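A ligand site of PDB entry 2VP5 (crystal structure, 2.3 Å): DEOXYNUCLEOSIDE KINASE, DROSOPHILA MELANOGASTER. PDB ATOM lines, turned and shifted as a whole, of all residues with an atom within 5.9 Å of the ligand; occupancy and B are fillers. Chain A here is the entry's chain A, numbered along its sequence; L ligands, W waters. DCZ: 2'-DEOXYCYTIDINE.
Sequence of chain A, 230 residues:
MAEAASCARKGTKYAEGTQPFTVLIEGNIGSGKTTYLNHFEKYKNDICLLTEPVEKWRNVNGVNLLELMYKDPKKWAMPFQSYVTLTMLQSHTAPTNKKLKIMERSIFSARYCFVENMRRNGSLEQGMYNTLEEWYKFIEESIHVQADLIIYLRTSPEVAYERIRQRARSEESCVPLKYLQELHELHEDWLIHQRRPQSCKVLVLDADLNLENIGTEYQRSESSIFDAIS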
ATOM      1  N   ILE A  29      -4.209  -4.597  -1.436  1.00  0.00           N
ATOM      2  CA  ILE A  29      -5.455  -3.979  -1.855  1.00  0.00           C
ATOM      3  C   ILE A  29      -5.313  -3.715  -3.358  1.00  0.00           C
ATOM      4  O   ILE A  29      -4.322  -3.156  -3.789  1.00  0.00           O
ATOM      5  CB  ILE A  29      -5.749  -2.631  -1.106  1.00  0.00           C
ATOM      6  CG1 ILE A  29      -5.682  -2.817   0.415  1.00  0.00           C
ATOM      7  CG2 ILE A  29      -7.110  -2.073  -1.503  1.00  0.00           C
ATOM      8  CD1 ILE A  29      -5.626  -1.511   1.219  1.00  0.00           C
ATOM      9  N   LYS A  33      -8.013  -9.991  -6.179  1.00  0.00           N
ATOM     10  CA  LYS A  33      -8.481 -11.187  -5.438  1.00  0.00           C
ATOM     11  C   LYS A  33      -9.944 -11.522  -5.650  1.00  0.00           C
ATOM     12  O   LYS A  33     -10.303 -12.682  -5.775  1.00  0.00           O
ATOM     13  CB  LYS A  33      -8.200 -11.038  -3.944  1.00  0.00           C
ATOM     14  CG  LYS A  33      -6.720 -10.866  -3.615  1.00  0.00           C
ATOM     15  CD  LYS A  33      -6.431 -11.041  -2.128  1.00  0.00           C
ATOM     16  CE  LYS A  33      -7.071  -9.981  -1.262  1.00  0.00           C
ATOM     17  NZ  LYS A  33      -6.860  -8.576  -1.739  1.00  0.00           N
ATOM     18  N   GLU A  52     -13.853 -12.446   1.517  1.00  0.00           N
ATOM     19  CA  GLU A  52     -13.480 -11.589   2.640  1.00  0.00           C
ATOM     20  C   GLU A  52     -14.733 -10.892   3.205  1.00  0.00           C
ATOM     21  O   GLU A  52     -15.502 -10.324   2.451  1.00  0.00           O
ATOM     22  CB  GLU A  52     -12.458 -10.539   2.212  1.00  0.00           C
ATOM     23  CG  GLU A  52     -11.610  -9.997   3.354  1.00  0.00           C
ATOM     24  CD  GLU A  52     -10.616  -8.946   2.916  1.00  0.00           C
ATOM     25  OE1 GLU A  52     -10.872  -8.220   1.944  1.00  0.00           O
ATOM     26  OE2 GLU A  52      -9.567  -8.827   3.585  1.00  0.00           O
ATOM     27  N   VAL A  54     -16.127  -8.258   4.107  1.00  0.00           N
ATOM     28  CA  VAL A  54     -16.305  -6.794   4.015  1.00  0.00           C
ATOM     29  C   VAL A  54     -17.735  -6.349   4.411  1.00  0.00           C
ATOM     30  O   VAL A  54     -17.919  -5.293   5.014  1.00  0.00           O
ATOM     31  CB  VAL A  54     -15.996  -6.266   2.582  1.00  0.00           C
ATOM     32  CG1 VAL A  54     -16.129  -4.763   2.522  1.00  0.00           C
ATOM     33  CG2 VAL A  54     -14.608  -6.680   2.159  1.00  0.00           C
ATOM     34  N   TRP A  57     -17.999  -6.079   8.102  1.00  0.00           N
ATOM     35  CA  TRP A  57     -17.248  -4.926   8.600  1.00  0.00           C
ATOM     36  C   TRP A  57     -17.988  -3.614   8.371  1.00  0.00           C
ATOM     37  O   TRP A  57     -17.822  -2.660   9.142  1.00  0.00           O
ATOM     38  CB  TRP A  57     -15.863  -4.836   7.934  1.00  0.00           C
ATOM     39  CG  TRP A  57     -15.004  -6.088   8.006  1.00  0.00           C
ATOM     40  CD1 TRP A  57     -15.146  -7.147   8.861  1.00  0.00           C
ATOM     41  CD2 TRP A  57     -13.845  -6.365   7.208  1.00  0.00           C
ATOM     42  NE1 TRP A  57     -14.163  -8.080   8.633  1.00  0.00           N
ATOM     43  CE2 TRP A  57     -13.345  -7.624   7.628  1.00  0.00           C
ATOM     44  CE3 TRP A  57     -13.178  -5.679   6.183  1.00  0.00           C
ATOM     45  CZ2 TRP A  57     -12.220  -8.212   7.052  1.00  0.00           C
ATOM     46  CZ3 TRP A  57     -12.046  -6.257   5.619  1.00  0.00           C
ATOM     47  CH2 TRP A  57     -11.585  -7.522   6.058  1.00  0.00           C
ATOM     48  N   LEU A  66     -15.117  -0.200   8.729  1.00  0.00           N
ATOM     49  CA  LEU A  66     -14.181  -0.013   7.621  1.00  0.00           C
ATOM     50  C   LEU A  66     -14.080   1.457   7.229  1.00  0.00           C
ATOM     51  O   LEU A  66     -12.986   1.994   7.119  1.00  0.00           O
ATOM     52  CB  LEU A  66     -14.585  -0.865   6.402  1.00  0.00           C
ATOM     53  CG  LEU A  66     -13.660  -0.867   5.173  1.00  0.00           C
ATOM     54  CD1 LEU A  66     -12.213  -1.295   5.521  1.00  0.00           C
ATOM     55  CD2 LEU A  66     -14.217  -1.740   4.065  1.00  0.00           C
ATOM     56  N   MET A  69     -12.443   3.357  10.213  1.00  0.00           N
ATOM     57  CA  MET A  69     -11.011   3.135  10.218  1.00  0.00           C
ATOM     58  C   MET A  69     -10.302   4.008   9.187  1.00  0.00           C
ATOM     59  O   MET A  69      -9.340   4.691   9.528  1.00  0.00           O
ATOM     60  CB  MET A  69     -10.692   1.647  10.010  1.00  0.00           C
ATOM     61  CG  MET A  69      -9.197   1.307   9.974  1.00  0.00           C
ATOM     62  SD  MET A  69      -8.407   1.514   8.351  1.00  0.00           S
ATOM     63  CE  MET A  69      -9.256   0.281   7.374  1.00  0.00           C
ATOM     64  N   TYR A  70     -10.796   4.026   7.946  1.00  0.00           N
ATOM     65  CA  TYR A  70     -10.194   4.823   6.877  1.00  0.00           C
ATOM     66  C   TYR A  70     -10.293   6.326   7.092  1.00  0.00           C
ATOM     67  O   TYR A  70      -9.390   7.078   6.729  1.00  0.00           O
ATOM     68  CB  TYR A  70     -10.757   4.453   5.504  1.00  0.00           C
ATOM     69  CG  TYR A  70     -10.031   3.306   4.876  1.00  0.00           C
ATOM     70  CD1 TYR A  70     -10.713   2.183   4.429  1.00  0.00           C
ATOM     71  CD2 TYR A  70      -8.653   3.337   4.732  1.00  0.00           C
ATOM     72  CE1 TYR A  70     -10.034   1.134   3.861  1.00  0.00           C
ATOM     73  CE2 TYR A  70      -7.976   2.289   4.173  1.00  0.00           C
ATOM     74  CZ  TYR A  70      -8.663   1.198   3.743  1.00  0.00           C
ATOM     75  OH  TYR A  70      -7.953   0.168   3.182  1.00  0.00           O
ATOM     76  N   PHE A  80     -11.572  -1.836  14.635  1.00  0.00           N
ATOM     77  CA  PHE A  80     -11.619  -2.441  13.297  1.00  0.00           C
ATOM     78  C   PHE A  80     -10.817  -3.734  13.184  1.00  0.00           C
ATOM     79  O   PHE A  80     -11.359  -4.754  12.773  1.00  0.00           O
ATOM     80  CB  PHE A  80     -11.182  -1.462  12.208  1.00  0.00           C
ATOM     81  CG  PHE A  80     -11.162  -2.066  10.828  1.00  0.00           C
ATOM     82  CD1 PHE A  80     -12.364  -2.383  10.182  1.00  0.00           C
ATOM     83  CD2 PHE A  80      -9.957  -2.324  10.182  1.00  0.00           C
ATOM     84  CE1 PHE A  80     -12.358  -2.957   8.911  1.00  0.00           C
ATOM     85  CE2 PHE A  80      -9.951  -2.897   8.910  1.00  0.00           C
ATOM     86  CZ  PHE A  80     -11.137  -3.215   8.279  1.00  0.00           C
ATOM     87  N   GLN A  81      -9.537  -3.705  13.558  1.00  0.00           N
ATOM     88  CA  GLN A  81      -8.684  -4.895  13.399  1.00  0.00           C
ATOM     89  C   GLN A  81      -9.089  -6.008  14.343  1.00  0.00           C
ATOM     90  O   GLN A  81      -8.885  -7.183  14.044  1.00  0.00           O
ATOM     91  CB  GLN A  81      -7.189  -4.565  13.580  1.00  0.00           C
ATOM     92  CG  GLN A  81      -6.557  -3.743  12.455  1.00  0.00           C
ATOM     93  CD  GLN A  81      -6.615  -4.411  11.077  1.00  0.00           C
ATOM     94  OE1 GLN A  81      -6.727  -5.629  10.965  1.00  0.00           O
ATOM     95  NE2 GLN A  81      -6.555  -3.604  10.021  1.00  0.00           N
ATOM     96  N   VAL A  84     -11.919  -7.489  12.532  1.00  0.00           N
ATOM     97  CA  VAL A  84     -11.343  -8.299  11.450  1.00  0.00           C
ATOM     98  C   VAL A  84     -10.907  -9.656  11.985  1.00  0.00           C
ATOM     99  O   VAL A  84     -11.295 -10.698  11.426  1.00  0.00           O
ATOM    100  CB  VAL A  84     -10.167  -7.587  10.705  1.00  0.00           C
ATOM    101  CG1 VAL A  84      -9.512  -8.537   9.716  1.00  0.00           C
ATOM    102  CG2 VAL A  84     -10.675  -6.340   9.988  1.00  0.00           C
ATOM    103  N   GLU A 104     -10.609 -15.952   0.929  1.00  0.00           N
ATOM    104  CA  GLU A 104     -10.039 -14.661   0.593  1.00  0.00           C
ATOM    105  C   GLU A 104      -9.453 -13.970   1.845  1.00  0.00           C
ATOM    106  O   GLU A 104     -10.186 -13.535   2.745  1.00  0.00           O
ATOM    107  CB  GLU A 104     -11.059 -13.767  -0.087  1.00  0.00           C
ATOM    108  CG  GLU A 104     -10.443 -12.540  -0.666  1.00  0.00           C
ATOM    109  CD  GLU A 104     -11.459 -11.576  -1.224  1.00  0.00           C
ATOM    110  OE1 GLU A 104     -12.673 -11.890  -1.198  1.00  0.00           O
ATOM    111  OE2 GLU A 104     -11.036 -10.496  -1.683  1.00  0.00           O
ATOM    112  N   ARG A 105      -8.122 -13.891   1.882  1.00  0.00           N
ATOM    113  CA  ARG A 105      -7.360 -13.431   3.046  1.00  0.00           C
ATOM    114  C   ARG A 105      -7.516 -14.338   4.283  1.00  0.00           C
ATOM    115  O   ARG A 105      -8.140 -15.406   4.209  1.00  0.00           O
ATOM    116  CB  ARG A 105      -7.632 -11.958   3.366  1.00  0.00           C
ATOM    117  CG  ARG A 105      -7.038 -11.006   2.343  1.00  0.00           C
ATOM    118  CD  ARG A 105      -6.477  -9.766   3.012  1.00  0.00           C
ATOM    119  NE  ARG A 105      -5.814  -8.903   2.052  1.00  0.00           N
ATOM    120  CZ  ARG A 105      -6.337  -7.789   1.556  1.00  0.00           C
ATOM    121  NH1 ARG A 105      -7.549  -7.402   1.923  1.00  0.00           N
ATOM    122  NH2 ARG A 105      -5.645  -7.063   0.682  1.00  0.00           N
ATOM    123  N   SER A 106      -6.927 -13.910   5.394  1.00  0.00           N
ATOM    124  CA  SER A 106      -6.796 -14.751   6.569  1.00  0.00           C
ATOM    125  C   SER A 106      -6.434 -13.945   7.811  1.00  0.00           C
ATOM    126  O   SER A 106      -6.163 -12.733   7.733  1.00  0.00           O
ATOM    127  CB  SER A 106      -5.744 -15.830   6.337  1.00  0.00           C
ATOM    128  OG  SER A 106      -4.469 -15.246   6.229  1.00  0.00           O
ATOM    129  N   SER A 109      -2.639 -12.525   7.311  1.00  0.00           N
ATOM    130  CA  SER A 109      -2.402 -11.235   6.675  1.00  0.00           C
ATOM    131  C   SER A 109      -2.860 -10.067   7.547  1.00  0.00           C
ATOM    132  O   SER A 109      -2.229  -8.996   7.538  1.00  0.00           O
ATOM    133  CB  SER A 109      -3.033 -11.149   5.286  1.00  0.00           C
ATOM    134  OG  SER A 109      -4.370 -11.574   5.315  1.00  0.00           O
ATOM    135  N   ALA A 110      -3.976 -10.244   8.247  1.00  0.00           N
ATOM    136  CA  ALA A 110      -4.386  -9.297   9.294  1.00  0.00           C
ATOM    137  C   ALA A 110      -3.239  -9.039  10.289  1.00  0.00           C
ATOM    138  O   ALA A 110      -2.857  -7.910  10.531  1.00  0.00           O
ATOM    139  CB  ALA A 110      -5.611  -9.796  10.023  1.00  0.00           C
ATOM    140  N   ARG A 111      -2.674 -10.102  10.826  1.00  0.00           N
ATOM    141  CA  ARG A 111      -1.609  -9.971  11.795  1.00  0.00           C
ATOM    142  C   ARG A 111      -0.304  -9.459  11.176  1.00  0.00           C
ATOM    143  O   ARG A 111       0.244  -8.446  11.632  1.00  0.00           O
ATOM    144  CB  ARG A 111      -1.377 -11.311  12.474  1.00  0.00           C
ATOM    145  CG  ARG A 111      -0.386 -11.243  13.595  1.00  0.00           C
ATOM    146  CD  ARG A 111      -0.062 -12.610  14.148  1.00  0.00           C
ATOM    147  NE  ARG A 111       0.768 -12.494  15.348  1.00  0.00           N
ATOM    148  CZ  ARG A 111       1.121 -13.514  16.118  1.00  0.00           C
ATOM    149  NH1 ARG A 111       0.763 -14.749  15.821  1.00  0.00           N
ATOM    150  NH2 ARG A 111       1.863 -13.292  17.184  1.00  0.00           N
ATOM    151  N   PHE A 114      -1.477  -6.139   7.852  1.00  0.00           N
ATOM    152  CA  PHE A 114      -2.372  -4.997   8.129  1.00  0.00           C
ATOM    153  C   PHE A 114      -2.212  -4.414   9.538  1.00  0.00           C
ATOM    154  O   PHE A 114      -2.189  -3.197   9.696  1.00  0.00           O
ATOM    155  CB  PHE A 114      -3.838  -5.331   7.799  1.00  0.00           C
ATOM    156  CG  PHE A 114      -4.123  -5.448   6.322  1.00  0.00           C
ATOM    157  CD1 PHE A 114      -4.037  -6.682   5.673  1.00  0.00           C
ATOM    158  CD2 PHE A 114      -4.465  -4.327   5.567  1.00  0.00           C
ATOM    159  CE1 PHE A 114      -4.296  -6.792   4.310  1.00  0.00           C
ATOM    160  CE2 PHE A 114      -4.735  -4.415   4.208  1.00  0.00           C
ATOM    161  CZ  PHE A 114      -4.643  -5.649   3.572  1.00  0.00           C
ATOM    162  N   VAL A 115      -2.057  -5.271  10.543  1.00  0.00           N
ATOM    163  CA  VAL A 115      -1.845  -4.786  11.906  1.00  0.00           C
ATOM    164  C   VAL A 115      -0.415  -4.253  12.055  1.00  0.00           C
ATOM    165  O   VAL A 115      -0.206  -3.149  12.592  1.00  0.00           O
ATOM    166  CB  VAL A 115      -2.200  -5.862  12.989  1.00  0.00           C
ATOM    167  CG1 VAL A 115      -1.579  -5.518  14.341  1.00  0.00           C
ATOM    168  CG2 VAL A 115      -3.724  -6.035  13.110  1.00  0.00           C
ATOM    169  N   GLU A 172     -11.922   2.376   0.694  1.00  0.00           N
ATOM    170  CA  GLU A 172     -10.528   2.268   0.200  1.00  0.00           C
ATOM    171  C   GLU A 172     -10.012   3.420  -0.659  1.00  0.00           C
ATOM    172  O   GLU A 172      -8.788   3.647  -0.757  1.00  0.00           O
ATOM    173  CB  GLU A 172     -10.428   1.098  -0.768  1.00  0.00           C
ATOM    174  CG  GLU A 172     -10.391  -0.289  -0.212  1.00  0.00           C
ATOM    175  CD  GLU A 172     -10.339  -1.296  -1.329  1.00  0.00           C
ATOM    176  OE1 GLU A 172     -10.303  -0.868  -2.492  1.00  0.00           O
ATOM    177  OE2 GLU A 172     -10.316  -2.523  -1.058  1.00  0.00           O
ATOM    178  N   VAL A 175      -6.673   5.567  -0.388  1.00  0.00           N
ATOM    179  CA  VAL A 175      -5.413   5.089   0.169  1.00  0.00           C
ATOM    180  C   VAL A 175      -4.237   5.580  -0.702  1.00  0.00           C
ATOM    181  O   VAL A 175      -4.207   5.342  -1.904  1.00  0.00           O
ATOM    182  CB  VAL A 175      -5.362   3.535   0.408  1.00  0.00           C
ATOM    183  CG1 VAL A 175      -6.411   3.136   1.416  1.00  0.00           C
ATOM    184  CG2 VAL A 175      -5.533   2.750  -0.900  1.00  0.00           C
ATOM    185  N   TYR A 179       0.910   3.951   1.267  1.00  0.00           N
ATOM    186  CA  TYR A 179       0.244   2.914   2.053  1.00  0.00           C
ATOM    187  C   TYR A 179       0.267   1.560   1.354  1.00  0.00           C
ATOM    188  O   TYR A 179       0.589   0.549   1.965  1.00  0.00           O
ATOM    189  CB  TYR A 179      -1.209   3.351   2.326  1.00  0.00           C
ATOM    190  CG  TYR A 179      -2.012   2.476   3.263  1.00  0.00           C
ATOM    191  CD1 TYR A 179      -1.817   2.542   4.652  1.00  0.00           C
ATOM    192  CD2 TYR A 179      -2.995   1.633   2.773  1.00  0.00           C
ATOM    193  CE1 TYR A 179      -2.571   1.749   5.512  1.00  0.00           C
ATOM    194  CE2 TYR A 179      -3.755   0.849   3.620  1.00  0.00           C
ATOM    195  CZ  TYR A 179      -3.543   0.912   4.994  1.00  0.00           C
ATOM    196  OH  TYR A 179      -4.291   0.117   5.835  1.00  0.00           O
HETATM  197  N1  DCZ L   1      -8.416  -4.600   5.295  1.00  0.00           N
HETATM  198  C2  DCZ L   1      -7.811  -4.123   6.396  1.00  0.00           C
HETATM  199  N3  DCZ L   1      -7.301  -4.941   7.323  1.00  0.00           N
HETATM  200  C4  DCZ L   1      -7.384  -6.275   7.168  1.00  0.00           C
HETATM  201  C5  DCZ L   1      -8.002  -6.803   6.037  1.00  0.00           C
HETATM  202  C6  DCZ L   1      -8.522  -5.916   5.088  1.00  0.00           C
HETATM  203  O2  DCZ L   1      -7.687  -2.790   6.585  1.00  0.00           O
HETATM  204  N4  DCZ L   1      -6.851  -7.082   8.123  1.00  0.00           N
HETATM  205  C1' DCZ L   1      -8.950  -3.642   4.335  1.00  0.00           C
HETATM  206  C2' DCZ L   1      -8.131  -3.571   3.052  1.00  0.00           C
HETATM  207  C3' DCZ L   1      -9.164  -3.237   2.014  1.00  0.00           C
HETATM  208  C4' DCZ L   1     -10.525  -3.617   2.601  1.00  0.00           C
HETATM  209  O4' DCZ L   1     -10.273  -4.011   3.950  1.00  0.00           O
HETATM  210  O3' DCZ L   1      -9.143  -1.833   1.856  1.00  0.00           O
HETATM  211  C5' DCZ L   1     -11.179  -4.784   1.872  1.00  0.00           C
HETATM  212  O5' DCZ L   1     -10.207  -5.821   1.725  1.00  0.00           O
HETATM  213  O   HOH W   1      -9.163  -9.975   5.960  1.00  0.00           O
HETATM  214  O   HOH W   2      -8.158  -6.010  -0.724  1.00  0.00           O
HETATM  215  O   HOH W   3      -6.371  -1.077   4.758  1.00  0.00           O
HETATM  216  O   HOH W   4      -6.788  -9.747   6.905  1.00  0.00           O
HETATM  217  O   HOH W   5      -6.388  -1.247   8.312  1.00  0.00           O
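The side-chain carboxylate of Glu 52 sits at hydrogen-bond distance from an oxygen (O5') of the ligand, at 2.5 Å.
OE2 of Glu 172 sits close to O3' of the ligand.
OH of Tyr 70 is in hydrogen-bond range of O3' of the ligand (2.7 Å).
NH1 of Arg 105 sits at hydrogen-bond distance from O5' of the ligand (3.1 Å).
The side-chain amide nitrogen (NE2) of Gln 81 lies within hydrogen-bond range of a nitrogen (N3) of the ligand, 3.1 Å away.
N of Glu 52 sits at hydrogen-bond distance from OE1 of Glu 104.
The side-chain carboxylate (OE2) of Glu 52 is in salt-bridge range of the guanidinium group (NH1) of Arg 105 (3.0 Å).
The backbone NH (N) of Val 115 is in hydrogen-bond range of the backbone carbonyl oxygen (O) of Ala 110 (2.8 Å).
N of Phe 114 is in hydrogen-bond range of O of Ser 109 (3.0 Å).
Water W5 lies within hydrogen-bond range of an oxygen (O2) of the ligand (2.7 Å), the side-chain amide nitrogen (NE2) of Gln 81 (2.9 Å) and the side-chain sulfur (SD) of Met 69 (3.4 Å).
Water W3 lies within hydrogen-bond range of OH of Tyr 70 (2.6 Å), OH of Tyr 179 (2.6 Å) and O2 of the ligand (2.8 Å).
Water W4 lies within hydrogen-bond range of N4 of the ligand, N of Ala 110, O of Ser 106 and OG of Ser 109.
Water W2 lies within hydrogen-bond range of the side-chain amino group of Lys 33 (3.0 Å), the guanidinium group of Arg 105 (3.1 Å) and an oxygen (O5') of the ligand (3.2 Å).
Ile 29 touches the ligand.
CG2 of Val 54 touches C5' of the ligand (3.9 Å).
Trp 57 touches the ligand (CZ3 to O4', 3.3 Å).
Leu 66 touches the ligand.
Met 69 touches the ligand.
Phe 80 touches the ligand (CE2 to O2, 3.2 Å).
Val 84 touches the ligand (CG1 to N4, 3.4 Å).
Ala 110 touches the ligand (CA to N4, 3.5 Å).
Phe 114 touches the ligand.
Hydrophobic or aromatic side chains within 4 Å of the ligand: Ile 29, Val 54, Trp 57, Leu 66, Met 69, Tyr 70, Phe 80, Val 84, Ala 110 and Phe 114.
Of the 22 residues printed, 14 come within 4 Å of the ligand.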
